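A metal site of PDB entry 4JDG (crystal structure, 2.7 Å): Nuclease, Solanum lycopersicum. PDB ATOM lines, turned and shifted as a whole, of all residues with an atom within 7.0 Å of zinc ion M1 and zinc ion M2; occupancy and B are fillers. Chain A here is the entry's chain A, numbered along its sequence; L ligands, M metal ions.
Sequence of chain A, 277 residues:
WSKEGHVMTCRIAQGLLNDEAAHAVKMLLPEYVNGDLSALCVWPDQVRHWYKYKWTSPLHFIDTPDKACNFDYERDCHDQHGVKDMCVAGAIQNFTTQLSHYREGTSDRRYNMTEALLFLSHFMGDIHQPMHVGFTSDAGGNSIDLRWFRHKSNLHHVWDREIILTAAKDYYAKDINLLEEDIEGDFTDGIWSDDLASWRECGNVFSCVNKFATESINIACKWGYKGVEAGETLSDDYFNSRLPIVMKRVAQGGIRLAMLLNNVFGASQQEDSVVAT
The backbone carbonyl oxygen of His 122 lies close to a ring nitrogen (ND1) of His 6 (3.5 Å). The backbone carbonyl oxygen (O) of Gly 125 is in hydrogen-bond range of the indole nitrogen (NE1) of Trp 1 (2.9 Å). A ring nitrogen (ND1) of His 122 sits at hydrogen-bond distance from the backbone carbonyl oxygen of Cys 41, at 2.7 Å. A ring nitrogen (ND1) of His 132 is in hydrogen-bond range of the backbone carbonyl oxygen (O) of His 60, 2.7 Å away. The guanidinium group (NE) of Arg 48 is in salt-bridge range of the side-chain carboxylate (OD1) of Asp 45 (3.6 Å).
Four residues have an atom within 4 Å of zinc ion M1: Trp 1, His 6, His 122 and Asp 126. The nearest printed residue that does not touch zinc ion M1 is Asp 45 (4.03 Å).
Asp 45 touches zinc ion M2. The nearest printed residue that does not touch zinc ion M2 is His 6 (4.2 Å).
Zinc ion M1 is bound by NE2 of His 6 (1.9 Å), O of Trp 1 (2.1 Å), OD1 of Asp 126 (2.1 Å), O1 of the ligand (2.2 Å), O3 of the ligand (2.3 Å) and N of Trp 1 (2.3 Å).
Zinc ion M2 is bound by a ring nitrogen (NE2) of His 122 (2.2 Å), the side-chain carboxylate of Asp 126 (2.2 Å), an oxygen (O4) of the ligand (2.2 Å) and a ring nitrogen (ND1) of His 60 (2.2 Å). Slightly farther from zinc ion M2 lies an oxygen (O3) of the ligand (2.6 Å).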
ATOM      1  N   TRP A   1       9.129  -6.103  -8.867  1.00  0.00           N
ATOM      2  CA  TRP A   1       9.257  -4.828  -9.581  1.00  0.00           C
ATOM      3  C   TRP A   1      10.717  -4.386  -9.600  1.00  0.00           C
ATOM      4  O   TRP A   1      11.486  -4.753  -8.724  1.00  0.00           O
ATOM      5  CB  TRP A   1       8.449  -3.752  -8.879  1.00  0.00           C
ATOM      6  CG  TRP A   1       6.936  -3.952  -8.762  1.00  0.00           C
ATOM      7  CD1 TRP A   1       6.216  -3.949  -7.599  1.00  0.00           C
ATOM      8  CD2 TRP A   1       5.980  -4.093  -9.820  1.00  0.00           C
ATOM      9  NE1 TRP A   1       4.888  -4.097  -7.860  1.00  0.00           N
ATOM     10  CE2 TRP A   1       4.709  -4.185  -9.218  1.00  0.00           C
ATOM     11  CE3 TRP A   1       6.072  -4.145 -11.212  1.00  0.00           C
ATOM     12  CZ2 TRP A   1       3.539  -4.344  -9.965  1.00  0.00           C
ATOM     13  CZ3 TRP A   1       4.900  -4.297 -11.951  1.00  0.00           C
ATOM     14  CH2 TRP A   1       3.660  -4.403 -11.327  1.00  0.00           C
ATOM     15  N   SER A   2      11.088  -3.582 -10.601  1.00  0.00           N
ATOM     16  CA  SER A   2      12.368  -2.912 -10.634  1.00  0.00           C
ATOM     17  C   SER A   2      12.200  -1.610  -9.895  1.00  0.00           C
ATOM     18  O   SER A   2      11.133  -1.364  -9.340  1.00  0.00           O
ATOM     19  CB  SER A   2      12.794  -2.684 -12.059  1.00  0.00           C
ATOM     20  OG  SER A   2      12.841  -3.935 -12.719  1.00  0.00           O
ATOM     21  N   LYS A   3      13.241  -0.779  -9.891  1.00  0.00           N
ATOM     22  CA  LYS A   3      13.214   0.478  -9.133  1.00  0.00           C
ATOM     23  C   LYS A   3      11.829   1.084  -9.112  1.00  0.00           C
ATOM     24  O   LYS A   3      11.256   1.358  -8.040  1.00  0.00           O
ATOM     25  CB  LYS A   3      14.182   1.504  -9.737  1.00  0.00           C
ATOM     26  CG  LYS A   3      15.633   1.038  -9.774  1.00  0.00           C
ATOM     27  CD  LYS A   3      16.566   2.098  -9.198  1.00  0.00           C
ATOM     28  CE  LYS A   3      17.757   1.460  -8.516  1.00  0.00           C
ATOM     29  NZ  LYS A   3      18.589   2.399  -7.732  1.00  0.00           N
ATOM     30  N   GLY A   5       8.497   0.302  -9.897  1.00  0.00           N
ATOM     31  CA  GLY A   5       7.335  -0.287  -9.207  1.00  0.00           C
ATOM     32  C   GLY A   5       7.438  -0.149  -7.700  1.00  0.00           C
ATOM     33  O   GLY A   5       6.493   0.305  -7.024  1.00  0.00           O
ATOM     34  N   HIS A   6       8.603  -0.491  -7.162  1.00  0.00           N
ATOM     35  CA  HIS A   6       8.802  -0.351  -5.733  1.00  0.00           C
ATOM     36  C   HIS A   6       8.652   1.088  -5.259  1.00  0.00           C
ATOM     37  O   HIS A   6       7.993   1.337  -4.250  1.00  0.00           O
ATOM     38  CB  HIS A   6      10.140  -0.927  -5.329  1.00  0.00           C
ATOM     39  CG  HIS A   6      10.214  -2.399  -5.526  1.00  0.00           C
ATOM     40  ND1 HIS A   6       9.506  -3.284  -4.736  1.00  0.00           N
ATOM     41  CD2 HIS A   6      10.872  -3.158  -6.433  1.00  0.00           C
ATOM     42  CE1 HIS A   6       9.732  -4.515  -5.160  1.00  0.00           C
ATOM     43  NE2 HIS A   6      10.568  -4.458  -6.170  1.00  0.00           N
ATOM     44  N   CYS A  41      13.302   1.220  -0.718  1.00  0.00           N
ATOM     45  CA  CYS A  41      12.520   0.011  -1.056  1.00  0.00           C
ATOM     46  C   CYS A  41      13.232  -0.949  -2.003  1.00  0.00           C
ATOM     47  O   CYS A  41      12.854  -2.098  -2.089  1.00  0.00           O
ATOM     48  CB  CYS A  41      11.130   0.377  -1.610  1.00  0.00           C
ATOM     49  SG  CYS A  41      10.043   0.898  -0.259  1.00  0.00           S
ATOM     50  N   VAL A  42      14.228  -0.480  -2.741  1.00  0.00           N
ATOM     51  CA  VAL A  42      14.977  -1.363  -3.645  1.00  0.00           C
ATOM     52  C   VAL A  42      16.074  -2.105  -2.878  1.00  0.00           C
ATOM     53  O   VAL A  42      16.542  -3.136  -3.310  1.00  0.00           O
ATOM     54  CB  VAL A  42      15.559  -0.571  -4.851  1.00  0.00           C
ATOM     55  CG1 VAL A  42      16.343  -1.467  -5.786  1.00  0.00           C
ATOM     56  CG2 VAL A  42      14.424   0.034  -5.635  1.00  0.00           C
ATOM     57  N   PRO A  44      16.586  -4.370  -0.760  1.00  0.00           N
ATOM     58  CA  PRO A  44      16.695  -5.825  -0.794  1.00  0.00           C
ATOM     59  C   PRO A  44      17.180  -6.393  -2.107  1.00  0.00           C
ATOM     60  O   PRO A  44      17.592  -7.547  -2.149  1.00  0.00           O
ATOM     61  CB  PRO A  44      15.263  -6.289  -0.541  1.00  0.00           C
ATOM     62  CG  PRO A  44      14.680  -5.192   0.261  1.00  0.00           C
ATOM     63  CD  PRO A  44      15.251  -3.938  -0.308  1.00  0.00           C
ATOM     64  N   ASP A  45      17.073  -5.618  -3.179  1.00  0.00           N
ATOM     65  CA  ASP A  45      17.393  -6.109  -4.520  1.00  0.00           C
ATOM     66  C   ASP A  45      18.884  -5.967  -4.774  1.00  0.00           C
ATOM     67  O   ASP A  45      19.439  -6.634  -5.645  1.00  0.00           O
ATOM     68  CB  ASP A  45      16.622  -5.306  -5.585  1.00  0.00           C
ATOM     69  CG  ASP A  45      15.548  -6.104  -6.288  1.00  0.00           C
ATOM     70  OD1 ASP A  45      15.554  -7.349  -6.268  1.00  0.00           O
ATOM     71  OD2 ASP A  45      14.703  -5.461  -6.937  1.00  0.00           O
ATOM     72  N   ARG A  48      20.543  -8.796  -2.452  1.00  0.00           N
ATOM     73  CA  ARG A  48      20.195 -10.072  -3.076  1.00  0.00           C
ATOM     74  C   ARG A  48      21.438 -10.856  -3.553  1.00  0.00           C
ATOM     75  O   ARG A  48      21.415 -12.088  -3.609  1.00  0.00           O
ATOM     76  CB  ARG A  48      19.291  -9.717  -4.276  1.00  0.00           C
ATOM     77  CG  ARG A  48      18.652 -10.848  -5.059  1.00  0.00           C
ATOM     78  CD  ARG A  48      17.920 -10.263  -6.277  1.00  0.00           C
ATOM     79  NE  ARG A  48      16.576 -10.795  -6.455  1.00  0.00           N
ATOM     80  CZ  ARG A  48      16.296 -12.067  -6.758  1.00  0.00           C
ATOM     81  NH1 ARG A  48      17.266 -12.969  -6.883  1.00  0.00           N
ATOM     82  NH2 ARG A  48      15.033 -12.452  -6.913  1.00  0.00           N
ATOM     83  N   LEU A  59      13.278 -15.472  -1.514  1.00  0.00           N
ATOM     84  CA  LEU A  59      12.183 -14.740  -0.872  1.00  0.00           C
ATOM     85  C   LEU A  59      11.543 -13.693  -1.776  1.00  0.00           C
ATOM     86  O   LEU A  59      10.697 -12.922  -1.330  1.00  0.00           O
ATOM     87  CB  LEU A  59      12.687 -14.044   0.423  1.00  0.00           C
ATOM     88  CG  LEU A  59      13.321 -14.844   1.562  1.00  0.00           C
ATOM     89  CD1 LEU A  59      13.563 -13.968   2.788  1.00  0.00           C
ATOM     90  CD2 LEU A  59      12.418 -15.989   1.949  1.00  0.00           C
ATOM     91  N   HIS A  60      11.960 -13.583  -3.019  1.00  0.00           N
ATOM     92  CA  HIS A  60      11.405 -12.528  -3.887  1.00  0.00           C
ATOM     93  C   HIS A  60      10.212 -13.022  -4.677  1.00  0.00           C
ATOM     94  O   HIS A  60       9.388 -12.220  -5.156  1.00  0.00           O
ATOM     95  CB  HIS A  60      12.491 -12.016  -4.838  1.00  0.00           C
ATOM     96  CG  HIS A  60      13.474 -11.127  -4.149  1.00  0.00           C
ATOM     97  ND1 HIS A  60      13.673  -9.817  -4.513  1.00  0.00           N
ATOM     98  CD2 HIS A  60      14.295 -11.345  -3.098  1.00  0.00           C
ATOM     99  CE1 HIS A  60      14.565  -9.266  -3.711  1.00  0.00           C
ATOM    100  NE2 HIS A  60      14.968 -10.183  -2.852  1.00  0.00           N
ATOM    101  N   PHE A  61      10.099 -14.352  -4.789  1.00  0.00           N
ATOM    102  CA  PHE A  61       9.148 -14.957  -5.674  1.00  0.00           C
ATOM    103  C   PHE A  61       8.493 -16.221  -5.123  1.00  0.00           C
ATOM    104  O   PHE A  61       8.732 -16.634  -3.966  1.00  0.00           O
ATOM    105  CB  PHE A  61       9.846 -15.266  -6.988  1.00  0.00           C
ATOM    106  CG  PHE A  61      11.045 -16.130  -6.833  1.00  0.00           C
ATOM    107  CD1 PHE A  61      12.290 -15.577  -6.584  1.00  0.00           C
ATOM    108  CD2 PHE A  61      10.958 -17.506  -6.991  1.00  0.00           C
ATOM    109  CE1 PHE A  61      13.415 -16.392  -6.470  1.00  0.00           C
ATOM    110  CE2 PHE A  61      12.084 -18.321  -6.877  1.00  0.00           C
ATOM    111  CZ  PHE A  61      13.298 -17.767  -6.612  1.00  0.00           C
ATOM    112  N   HIS A 122       9.430  -4.007   0.469  1.00  0.00           N
ATOM    113  CA  HIS A 122       9.872  -4.485  -0.840  1.00  0.00           C
ATOM    114  C   HIS A 122       9.083  -5.698  -1.302  1.00  0.00           C
ATOM    115  O   HIS A 122       8.594  -5.725  -2.422  1.00  0.00           O
ATOM    116  CB  HIS A 122      11.343  -4.865  -0.796  1.00  0.00           C
ATOM    117  CG  HIS A 122      11.854  -5.373  -2.096  1.00  0.00           C
ATOM    118  ND1 HIS A 122      12.387  -4.540  -3.052  1.00  0.00           N
ATOM    119  CD2 HIS A 122      11.847  -6.624  -2.625  1.00  0.00           C
ATOM    120  CE1 HIS A 122      12.712  -5.265  -4.118  1.00  0.00           C
ATOM    121  NE2 HIS A 122      12.403  -6.526  -3.877  1.00  0.00           N
ATOM    122  N   PHE A 123       8.988  -6.709  -0.450  1.00  0.00           N
ATOM    123  CA  PHE A 123       8.283  -7.964  -0.777  1.00  0.00           C
ATOM    124  C   PHE A 123       6.767  -7.817  -0.922  1.00  0.00           C
ATOM    125  O   PHE A 123       6.110  -8.599  -1.618  1.00  0.00           O
ATOM    126  CB  PHE A 123       8.592  -9.021   0.268  1.00  0.00           C
ATOM    127  CG  PHE A 123      10.049  -9.417   0.336  1.00  0.00           C
ATOM    128  CD1 PHE A 123      10.699  -9.843  -0.783  1.00  0.00           C
ATOM    129  CD2 PHE A 123      10.723  -9.435   1.546  1.00  0.00           C
ATOM    130  CE1 PHE A 123      12.029 -10.224  -0.730  1.00  0.00           C
ATOM    131  CE2 PHE A 123      12.047  -9.817   1.612  1.00  0.00           C
ATOM    132  CZ  PHE A 123      12.704 -10.212   0.467  1.00  0.00           C
ATOM    133  N   GLY A 125       5.494  -5.344  -2.524  1.00  0.00           N
ATOM    134  CA  GLY A 125       5.464  -4.979  -3.938  1.00  0.00           C
ATOM    135  C   GLY A 125       5.750  -6.159  -4.852  1.00  0.00           C
ATOM    136  O   GLY A 125       5.130  -6.268  -5.919  1.00  0.00           O
ATOM    137  N   ASP A 126       6.678  -7.047  -4.455  1.00  0.00           N
ATOM    138  CA  ASP A 126       7.041  -8.183  -5.326  1.00  0.00           C
ATOM    139  C   ASP A 126       5.875  -9.172  -5.496  1.00  0.00           C
ATOM    140  O   ASP A 126       5.655  -9.681  -6.596  1.00  0.00           O
ATOM    141  CB  ASP A 126       8.287  -8.931  -4.817  1.00  0.00           C
ATOM    142  CG  ASP A 126       9.606  -8.397  -5.432  1.00  0.00           C
ATOM    143  OD1 ASP A 126       9.599  -7.378  -6.120  1.00  0.00           O
ATOM    144  OD2 ASP A 126      10.664  -9.021  -5.207  1.00  0.00           O
ATOM    145  N   GLN A 129       3.508  -8.202  -8.275  1.00  0.00           N
ATOM    146  CA  GLN A 129       4.039  -8.315  -9.640  1.00  0.00           C
ATOM    147  C   GLN A 129       3.651  -9.700 -10.128  1.00  0.00           C
ATOM    148  O   GLN A 129       4.240 -10.675  -9.689  1.00  0.00           O
ATOM    149  CB  GLN A 129       5.563  -8.143  -9.675  1.00  0.00           C
ATOM    150  CG  GLN A 129       6.088  -7.541 -10.967  1.00  0.00           C
ATOM    151  CD  GLN A 129       6.266  -8.556 -12.064  1.00  0.00           C
ATOM    152  OE1 GLN A 129       5.373  -9.329 -12.369  1.00  0.00           O
ATOM    153  NE2 GLN A 129       7.452  -8.564 -12.663  1.00  0.00           N
ATOM    154  N   HIS A 132       5.957 -12.634 -10.457  1.00  0.00           N
ATOM    155  CA  HIS A 132       6.665 -13.139  -9.276  1.00  0.00           C
ATOM    156  C   HIS A 132       6.032 -14.395  -8.698  1.00  0.00           C
ATOM    157  O   HIS A 132       6.584 -15.025  -7.791  1.00  0.00           O
ATOM    158  CB  HIS A 132       6.801 -12.049  -8.219  1.00  0.00           C
ATOM    159  CG  HIS A 132       7.970 -11.164  -8.479  1.00  0.00           C
ATOM    160  ND1 HIS A 132       9.047 -11.091  -7.621  1.00  0.00           N
ATOM    161  CD2 HIS A 132       8.291 -10.415  -9.559  1.00  0.00           C
ATOM    162  CE1 HIS A 132       9.946 -10.286  -8.138  1.00  0.00           C
ATOM    163  NE2 HIS A 132       9.517  -9.872  -9.321  1.00  0.00           N
ATOM    164  N   ASP A 160       8.281  -6.325 -14.856  1.00  0.00           N
ATOM    165  CA  ASP A 160       9.088  -5.626 -13.829  1.00  0.00           C
ATOM    166  C   ASP A 160       9.358  -4.171 -14.199  1.00  0.00           C
ATOM    167  O   ASP A 160       9.519  -3.323 -13.320  1.00  0.00           O
ATOM    168  CB  ASP A 160      10.436  -6.319 -13.621  1.00  0.00           C
ATOM    169  CG  ASP A 160      10.431  -7.294 -12.482  1.00  0.00           C
ATOM    170  OD1 ASP A 160      10.617  -6.870 -11.320  1.00  0.00           O
ATOM    171  OD2 ASP A 160      10.254  -8.496 -12.741  1.00  0.00           O
HETATM  172  P1  LIG L   1      12.500  -7.812  -8.306  1.00  0.00           P
HETATM  173  O1  LIG L   1      11.030  -7.625  -8.759  1.00  0.00           O
HETATM  174  O2  LIG L   1      13.405  -7.951  -9.547  1.00  0.00           O
HETATM  175  O3  LIG L   1      12.888  -6.580  -7.506  1.00  0.00           O
HETATM  176  O4  LIG L   1      12.734  -9.005  -7.360  1.00  0.00           O
HETATM  177 ZN    ZN M   1      10.723  -5.998  -7.240  1.00  0.00          ZN
HETATM  178 ZN    ZN M   2      12.632  -8.069  -5.372  1.00  0.00          ZN
HETATM  179 ZN    ZN M   3      11.278  -9.218 -10.767  1.00  0.00          ZN
